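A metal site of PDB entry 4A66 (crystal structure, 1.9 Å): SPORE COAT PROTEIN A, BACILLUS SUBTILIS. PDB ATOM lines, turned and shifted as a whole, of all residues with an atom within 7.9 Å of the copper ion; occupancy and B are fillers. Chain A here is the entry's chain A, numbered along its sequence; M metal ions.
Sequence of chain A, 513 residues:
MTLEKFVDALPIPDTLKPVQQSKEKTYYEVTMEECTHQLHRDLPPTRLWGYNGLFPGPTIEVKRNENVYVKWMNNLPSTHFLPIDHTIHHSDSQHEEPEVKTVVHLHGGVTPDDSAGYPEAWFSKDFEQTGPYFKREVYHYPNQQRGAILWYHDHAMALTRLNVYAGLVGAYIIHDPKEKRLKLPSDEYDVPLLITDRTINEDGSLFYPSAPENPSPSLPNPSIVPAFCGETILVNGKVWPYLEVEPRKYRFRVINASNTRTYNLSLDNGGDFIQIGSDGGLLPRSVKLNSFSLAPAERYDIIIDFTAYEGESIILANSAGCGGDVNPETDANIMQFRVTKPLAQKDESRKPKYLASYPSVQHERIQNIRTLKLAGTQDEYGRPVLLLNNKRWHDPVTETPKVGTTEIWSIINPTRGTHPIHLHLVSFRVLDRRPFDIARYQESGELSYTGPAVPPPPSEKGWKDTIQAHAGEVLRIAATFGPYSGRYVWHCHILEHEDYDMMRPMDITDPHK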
ATOM      1  N   PRO A 226     -11.619 -20.517  17.293  1.00  0.00           N
ATOM      2  CA  PRO A 226     -10.337 -20.157  16.643  1.00  0.00           C
ATOM      3  C   PRO A 226     -10.031 -20.929  15.355  1.00  0.00           C
ATOM      4  O   PRO A 226      -8.997 -20.679  14.730  1.00  0.00           O
ATOM      5  CB  PRO A 226      -9.288 -20.518  17.722  1.00  0.00           C
ATOM      6  CG  PRO A 226      -9.946 -21.580  18.555  1.00  0.00           C
ATOM      7  CD  PRO A 226     -11.450 -21.479  18.405  1.00  0.00           C
ATOM      8  N   LEU A 374       4.147 -13.646  14.981  1.00  0.00           N
ATOM      9  CA  LEU A 374       2.802 -14.160  15.033  1.00  0.00           C
ATOM     10  C   LEU A 374       2.575 -14.527  16.481  1.00  0.00           C
ATOM     11  O   LEU A 374       3.174 -15.467  17.000  1.00  0.00           O
ATOM     12  CB  LEU A 374       2.640 -15.376  14.108  1.00  0.00           C
ATOM     13  CG  LEU A 374       3.080 -15.148  12.654  1.00  0.00           C
ATOM     14  CD1 LEU A 374       2.758 -16.396  11.756  1.00  0.00           C
ATOM     15  CD2 LEU A 374       2.460 -13.898  12.068  1.00  0.00           C
ATOM     16  N   LEU A 386      -5.531 -13.871  18.404  1.00  0.00           N
ATOM     17  CA  LEU A 386      -4.310 -13.947  17.612  1.00  0.00           C
ATOM     18  C   LEU A 386      -3.979 -12.571  17.089  1.00  0.00           C
ATOM     19  O   LEU A 386      -4.839 -11.900  16.540  1.00  0.00           O
ATOM     20  CB  LEU A 386      -4.450 -14.947  16.470  1.00  0.00           C
ATOM     21  CG  LEU A 386      -4.308 -16.401  16.955  1.00  0.00           C
ATOM     22  CD1 LEU A 386      -4.933 -17.347  15.965  1.00  0.00           C
ATOM     23  CD2 LEU A 386      -2.828 -16.766  17.212  1.00  0.00           C
ATOM     24  N   LEU A 388      -0.923  -9.948  15.179  1.00  0.00           N
ATOM     25  CA  LEU A 388       0.335  -9.733  14.471  1.00  0.00           C
ATOM     26  C   LEU A 388       1.117  -8.693  15.278  1.00  0.00           C
ATOM     27  O   LEU A 388       0.558  -7.628  15.559  1.00  0.00           O
ATOM     28  CB  LEU A 388       0.060  -9.218  13.055  1.00  0.00           C
ATOM     29  CG  LEU A 388      -0.812 -10.186  12.235  1.00  0.00           C
ATOM     30  CD1 LEU A 388      -1.323  -9.500  10.970  1.00  0.00           C
ATOM     31  CD2 LEU A 388      -0.064 -11.436  11.898  1.00  0.00           C
ATOM     32  N   ASN A 413       7.255 -17.281  13.505  1.00  0.00           N
ATOM     33  CA  ASN A 413       6.106 -18.018  13.987  1.00  0.00           C
ATOM     34  C   ASN A 413       6.456 -18.913  15.188  1.00  0.00           C
ATOM     35  O   ASN A 413       6.874 -20.050  14.992  1.00  0.00           O
ATOM     36  CB  ASN A 413       5.446 -18.869  12.869  1.00  0.00           C
ATOM     37  CG  ASN A 413       4.184 -19.578  13.340  1.00  0.00           C
ATOM     38  OD1 ASN A 413       3.764 -19.391  14.477  1.00  0.00           O
ATOM     39  ND2 ASN A 413       3.576 -20.384  12.481  1.00  0.00           N
ATOM     40  N   THR A 415       4.144 -20.018  17.298  1.00  0.00           N
ATOM     41  CA  THR A 415       2.891 -20.666  17.716  1.00  0.00           C
ATOM     42  C   THR A 415       2.967 -22.149  17.362  1.00  0.00           C
ATOM     43  O   THR A 415       3.937 -22.611  16.762  1.00  0.00           O
ATOM     44  CB  THR A 415       1.577 -20.021  17.067  1.00  0.00           C
ATOM     45  OG1 THR A 415       1.434 -20.435  15.681  1.00  0.00           O
ATOM     46  CG2 THR A 415       1.599 -18.482  17.167  1.00  0.00           C
ATOM     47  N   GLY A 417       0.855 -23.702  15.276  1.00  0.00           N
ATOM     48  CA  GLY A 417       0.309 -24.055  13.969  1.00  0.00           C
ATOM     49  C   GLY A 417       0.835 -23.212  12.825  1.00  0.00           C
ATOM     50  O   GLY A 417       1.528 -22.229  13.047  1.00  0.00           O
ATOM     51  N   THR A 418       0.507 -23.619  11.589  1.00  0.00           N
ATOM     52  CA  THR A 418       0.844 -22.850  10.375  1.00  0.00           C
ATOM     53  C   THR A 418      -0.158 -21.719  10.195  1.00  0.00           C
ATOM     54  O   THR A 418      -1.340 -21.916  10.479  1.00  0.00           O
ATOM     55  CB  THR A 418       0.806 -23.741   9.113  1.00  0.00           C
ATOM     56  OG1 THR A 418       1.805 -24.753   9.225  1.00  0.00           O
ATOM     57  CG2 THR A 418       1.128 -22.934   7.858  1.00  0.00           C
ATOM     58  N   HIS A 419       0.304 -20.533   9.768  1.00  0.00           N
ATOM     59  CA  HIS A 419      -0.620 -19.452   9.409  1.00  0.00           C
ATOM     60  C   HIS A 419      -0.370 -19.057   7.957  1.00  0.00           C
ATOM     61  O   HIS A 419       0.761 -18.785   7.614  1.00  0.00           O
ATOM     62  CB  HIS A 419      -0.441 -18.242  10.317  1.00  0.00           C
ATOM     63  CG  HIS A 419      -0.685 -18.559  11.755  1.00  0.00           C
ATOM     64  ND1 HIS A 419      -1.940 -18.488  12.328  1.00  0.00           N
ATOM     65  CD2 HIS A 419       0.155 -19.014  12.731  1.00  0.00           C
ATOM     66  CE1 HIS A 419      -1.854 -18.859  13.600  1.00  0.00           C
ATOM     67  NE2 HIS A 419      -0.598 -19.192  13.856  1.00  0.00           N
ATOM     68  N   PRO A 420      -1.433 -19.031   7.097  1.00  0.00           N
ATOM     69  CA  PRO A 420      -1.220 -18.578   5.718  1.00  0.00           C
ATOM     70  C   PRO A 420      -1.261 -17.043   5.673  1.00  0.00           C
ATOM     71  O   PRO A 420      -2.316 -16.441   5.719  1.00  0.00           O
ATOM     72  CB  PRO A 420      -2.389 -19.200   4.964  1.00  0.00           C
ATOM     73  CG  PRO A 420      -3.521 -19.211   5.995  1.00  0.00           C
ATOM     74  CD  PRO A 420      -2.826 -19.461   7.334  1.00  0.00           C
ATOM     75  N   ILE A 421      -0.090 -16.430   5.608  1.00  0.00           N
ATOM     76  CA  ILE A 421      -0.011 -14.977   5.723  1.00  0.00           C
ATOM     77  C   ILE A 421      -0.218 -14.366   4.356  1.00  0.00           C
ATOM     78  O   ILE A 421       0.433 -14.782   3.388  1.00  0.00           O
ATOM     79  CB  ILE A 421       1.376 -14.523   6.290  1.00  0.00           C
ATOM     80  CG1 ILE A 421       1.595 -15.096   7.710  1.00  0.00           C
ATOM     81  CG2 ILE A 421       1.473 -12.968   6.276  1.00  0.00           C
ATOM     82  CD1 ILE A 421       0.446 -14.709   8.720  1.00  0.00           C
ATOM     83  N   ALA A 469       3.301 -19.872   6.768  1.00  0.00           N
ATOM     84  CA  ALA A 469       4.332 -19.632   7.782  1.00  0.00           C
ATOM     85  C   ALA A 469       4.216 -20.733   8.819  1.00  0.00           C
ATOM     86  O   ALA A 469       3.333 -20.686   9.677  1.00  0.00           O
ATOM     87  CB  ALA A 469       4.159 -18.230   8.442  1.00  0.00           C
ATOM     88  N   HIS A 491      -2.584  -9.873   6.708  1.00  0.00           N
ATOM     89  CA  HIS A 491      -3.333 -10.678   7.678  1.00  0.00           C
ATOM     90  C   HIS A 491      -3.121 -12.177   7.473  1.00  0.00           C
ATOM     91  O   HIS A 491      -2.645 -12.609   6.399  1.00  0.00           O
ATOM     92  CB  HIS A 491      -4.848 -10.363   7.625  1.00  0.00           C
ATOM     93  CG  HIS A 491      -5.534 -10.697   6.318  1.00  0.00           C
ATOM     94  ND1 HIS A 491      -6.278 -11.855   6.139  1.00  0.00           N
ATOM     95  CD2 HIS A 491      -5.640  -9.995   5.172  1.00  0.00           C
ATOM     96  CE1 HIS A 491      -6.785 -11.853   4.913  1.00  0.00           C
ATOM     97  NE2 HIS A 491      -6.454 -10.713   4.325  1.00  0.00           N
ATOM     98  N   CYS A 492      -3.440 -12.946   8.497  1.00  0.00           N
ATOM     99  CA  CYS A 492      -3.591 -14.390   8.347  1.00  0.00           C
ATOM    100  C   CYS A 492      -4.905 -14.661   7.626  1.00  0.00           C
ATOM    101  O   CYS A 492      -5.897 -14.021   7.927  1.00  0.00           O
ATOM    102  CB  CYS A 492      -3.615 -15.073   9.696  1.00  0.00           C
ATOM    103  SG  CYS A 492      -3.915 -16.818   9.557  1.00  0.00           S
ATOM    104  N   HIS A 493      -4.909 -15.605   6.692  1.00  0.00           N
ATOM    105  CA  HIS A 493      -6.105 -15.876   5.886  1.00  0.00           C
ATOM    106  C   HIS A 493      -6.901 -17.088   6.427  1.00  0.00           C
ATOM    107  O   HIS A 493      -7.811 -17.593   5.757  1.00  0.00           O
ATOM    108  CB  HIS A 493      -5.757 -16.035   4.374  1.00  0.00           C
ATOM    109  CG  HIS A 493      -6.818 -15.480   3.451  1.00  0.00           C
ATOM    110  ND1 HIS A 493      -8.091 -16.033   3.367  1.00  0.00           N
ATOM    111  CD2 HIS A 493      -6.807 -14.442   2.573  1.00  0.00           C
ATOM    112  CE1 HIS A 493      -8.813 -15.343   2.485  1.00  0.00           C
ATOM    113  NE2 HIS A 493      -8.059 -14.376   1.985  1.00  0.00           N
ATOM    114  N   ILE A 494      -6.588 -17.531   7.635  1.00  0.00           N
ATOM    115  CA  ILE A 494      -7.539 -18.350   8.405  1.00  0.00           C
ATOM    116  C   ILE A 494      -8.533 -17.339   8.956  1.00  0.00           C
ATOM    117  O   ILE A 494      -8.180 -16.450   9.730  1.00  0.00           O
ATOM    118  CB  ILE A 494      -6.855 -19.172   9.520  1.00  0.00           C
ATOM    119  CG1 ILE A 494      -5.969 -20.242   8.886  1.00  0.00           C
ATOM    120  CG2 ILE A 494      -7.940 -19.811  10.512  1.00  0.00           C
ATOM    121  CD1 ILE A 494      -5.008 -20.919   9.815  1.00  0.00           C
ATOM    122  N   LEU A 495      -9.762 -17.421   8.471  1.00  0.00           N
ATOM    123  CA  LEU A 495     -10.749 -16.371   8.693  1.00  0.00           C
ATOM    124  C   LEU A 495     -11.105 -16.237  10.169  1.00  0.00           C
ATOM    125  O   LEU A 495     -11.341 -15.134  10.645  1.00  0.00           O
ATOM    126  CB  LEU A 495     -11.984 -16.602   7.823  1.00  0.00           C
ATOM    127  CG  LEU A 495     -11.681 -16.698   6.322  1.00  0.00           C
ATOM    128  CD1 LEU A 495     -13.027 -16.690   5.557  1.00  0.00           C
ATOM    129  CD2 LEU A 495     -10.802 -15.518   5.841  1.00  0.00           C
ATOM    130  N   GLU A 496     -11.106 -17.362  10.877  1.00  0.00           N
ATOM    131  CA  GLU A 496     -11.334 -17.366  12.315  1.00  0.00           C
ATOM    132  C   GLU A 496     -10.220 -16.623  13.051  1.00  0.00           C
ATOM    133  O   GLU A 496     -10.464 -16.069  14.140  1.00  0.00           O
ATOM    134  CB  GLU A 496     -11.445 -18.816  12.818  1.00  0.00           C
ATOM    135  CG  GLU A 496     -12.840 -19.484  12.543  1.00  0.00           C
ATOM    136  CD  GLU A 496     -13.120 -19.785  11.045  1.00  0.00           C
ATOM    137  OE1 GLU A 496     -12.137 -19.987  10.282  1.00  0.00           O
ATOM    138  OE2 GLU A 496     -14.317 -19.824  10.645  1.00  0.00           O
ATOM    139  N   HIS A 497      -9.019 -16.572  12.459  1.00  0.00           N
ATOM    140  CA  HIS A 497      -7.879 -15.848  13.067  1.00  0.00           C
ATOM    141  C   HIS A 497      -7.968 -14.391  12.640  1.00  0.00           C
ATOM    142  O   HIS A 497      -7.850 -13.502  13.469  1.00  0.00           O
ATOM    143  CB  HIS A 497      -6.548 -16.428  12.581  1.00  0.00           C
ATOM    144  CG  HIS A 497      -6.274 -17.821  13.031  1.00  0.00           C
ATOM    145  ND1 HIS A 497      -5.098 -18.487  12.722  1.00  0.00           N
ATOM    146  CD2 HIS A 497      -7.010 -18.673  13.798  1.00  0.00           C
ATOM    147  CE1 HIS A 497      -5.141 -19.698  13.255  1.00  0.00           C
ATOM    148  NE2 HIS A 497      -6.290 -19.837  13.905  1.00  0.00           N
ATOM    149  N   GLU A 498      -8.163 -14.167  11.338  1.00  0.00           N
ATOM    150  CA  GLU A 498      -8.367 -12.835  10.758  1.00  0.00           C
ATOM    151  C   GLU A 498      -9.357 -11.954  11.543  1.00  0.00           C
ATOM    152  O   GLU A 498      -9.100 -10.751  11.797  1.00  0.00           O
ATOM    153  CB  GLU A 498      -8.834 -13.000   9.306  1.00  0.00           C
ATOM    154  CG  GLU A 498      -9.143 -11.716   8.607  1.00  0.00           C
ATOM    155  CD  GLU A 498      -9.420 -11.920   7.133  1.00  0.00           C
ATOM    156  OE1 GLU A 498      -9.010 -12.966   6.569  1.00  0.00           O
ATOM    157  OE2 GLU A 498     -10.038 -11.025   6.550  1.00  0.00           O
ATOM    158  N   MET A 502      -6.201 -11.157  13.831  1.00  0.00           N
ATOM    159  CA  MET A 502      -4.892 -11.356  13.169  1.00  0.00           C
ATOM    160  C   MET A 502      -4.810 -10.650  11.807  1.00  0.00           C
ATOM    161  O   MET A 502      -4.608 -11.276  10.741  1.00  0.00           O
ATOM    162  CB  MET A 502      -4.567 -12.852  13.114  1.00  0.00           C
ATOM    163  CG  MET A 502      -3.087 -13.202  12.977  1.00  0.00           C
ATOM    164  SD  MET A 502      -2.870 -14.960  13.194  1.00  0.00           S
ATOM    165  CE  MET A 502      -1.145 -15.164  12.843  1.00  0.00           C
HETATM  166 CU    CU M   1      -3.639 -17.740  11.570  1.00  0.00          CU
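O of His 497 is in hydrogen-bond range of N of Met 502 (2.9 Å).
O of Pro 226 lies within hydrogen-bond range of NE2 of His 497.
ND1 of His 419 lies close to SD of Met 502 (3.7 Å).
NE2 of His 419 lies within hydrogen-bond range of OG1 of Thr 415 (3.0 Å).
The backbone carbonyl oxygen of His 419 sits at hydrogen-bond distance from the backbone NH of Ala 469 (2.9 Å).
The backbone carbonyl oxygen (O) of Met 502 is in hydrogen-bond range of the backbone NH (N) of Cys 492 (3.0 Å).
The side-chain sulfur (SG) of Cys 492 lies close to the backbone NH (N) of Ile 494.
The backbone NH (N) of Met 502 is in hydrogen-bond range of the backbone carbonyl oxygen (O) of Leu 386, at 3.1 Å.
The copper ion is bound by a ring nitrogen (ND1) of His 497 (2.0 Å), a ring nitrogen (ND1) of His 419 (2.0 Å) and the side-chain sulfur (SG) of Cys 492 (2.2 Å).
Ile 494 touches the copper ion (CD1 to CU, 3.9 Å).
Met 502 touches the copper ion.
The nearest printed residue that does not touch the copper ion is Leu 386 (4.6 Å).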
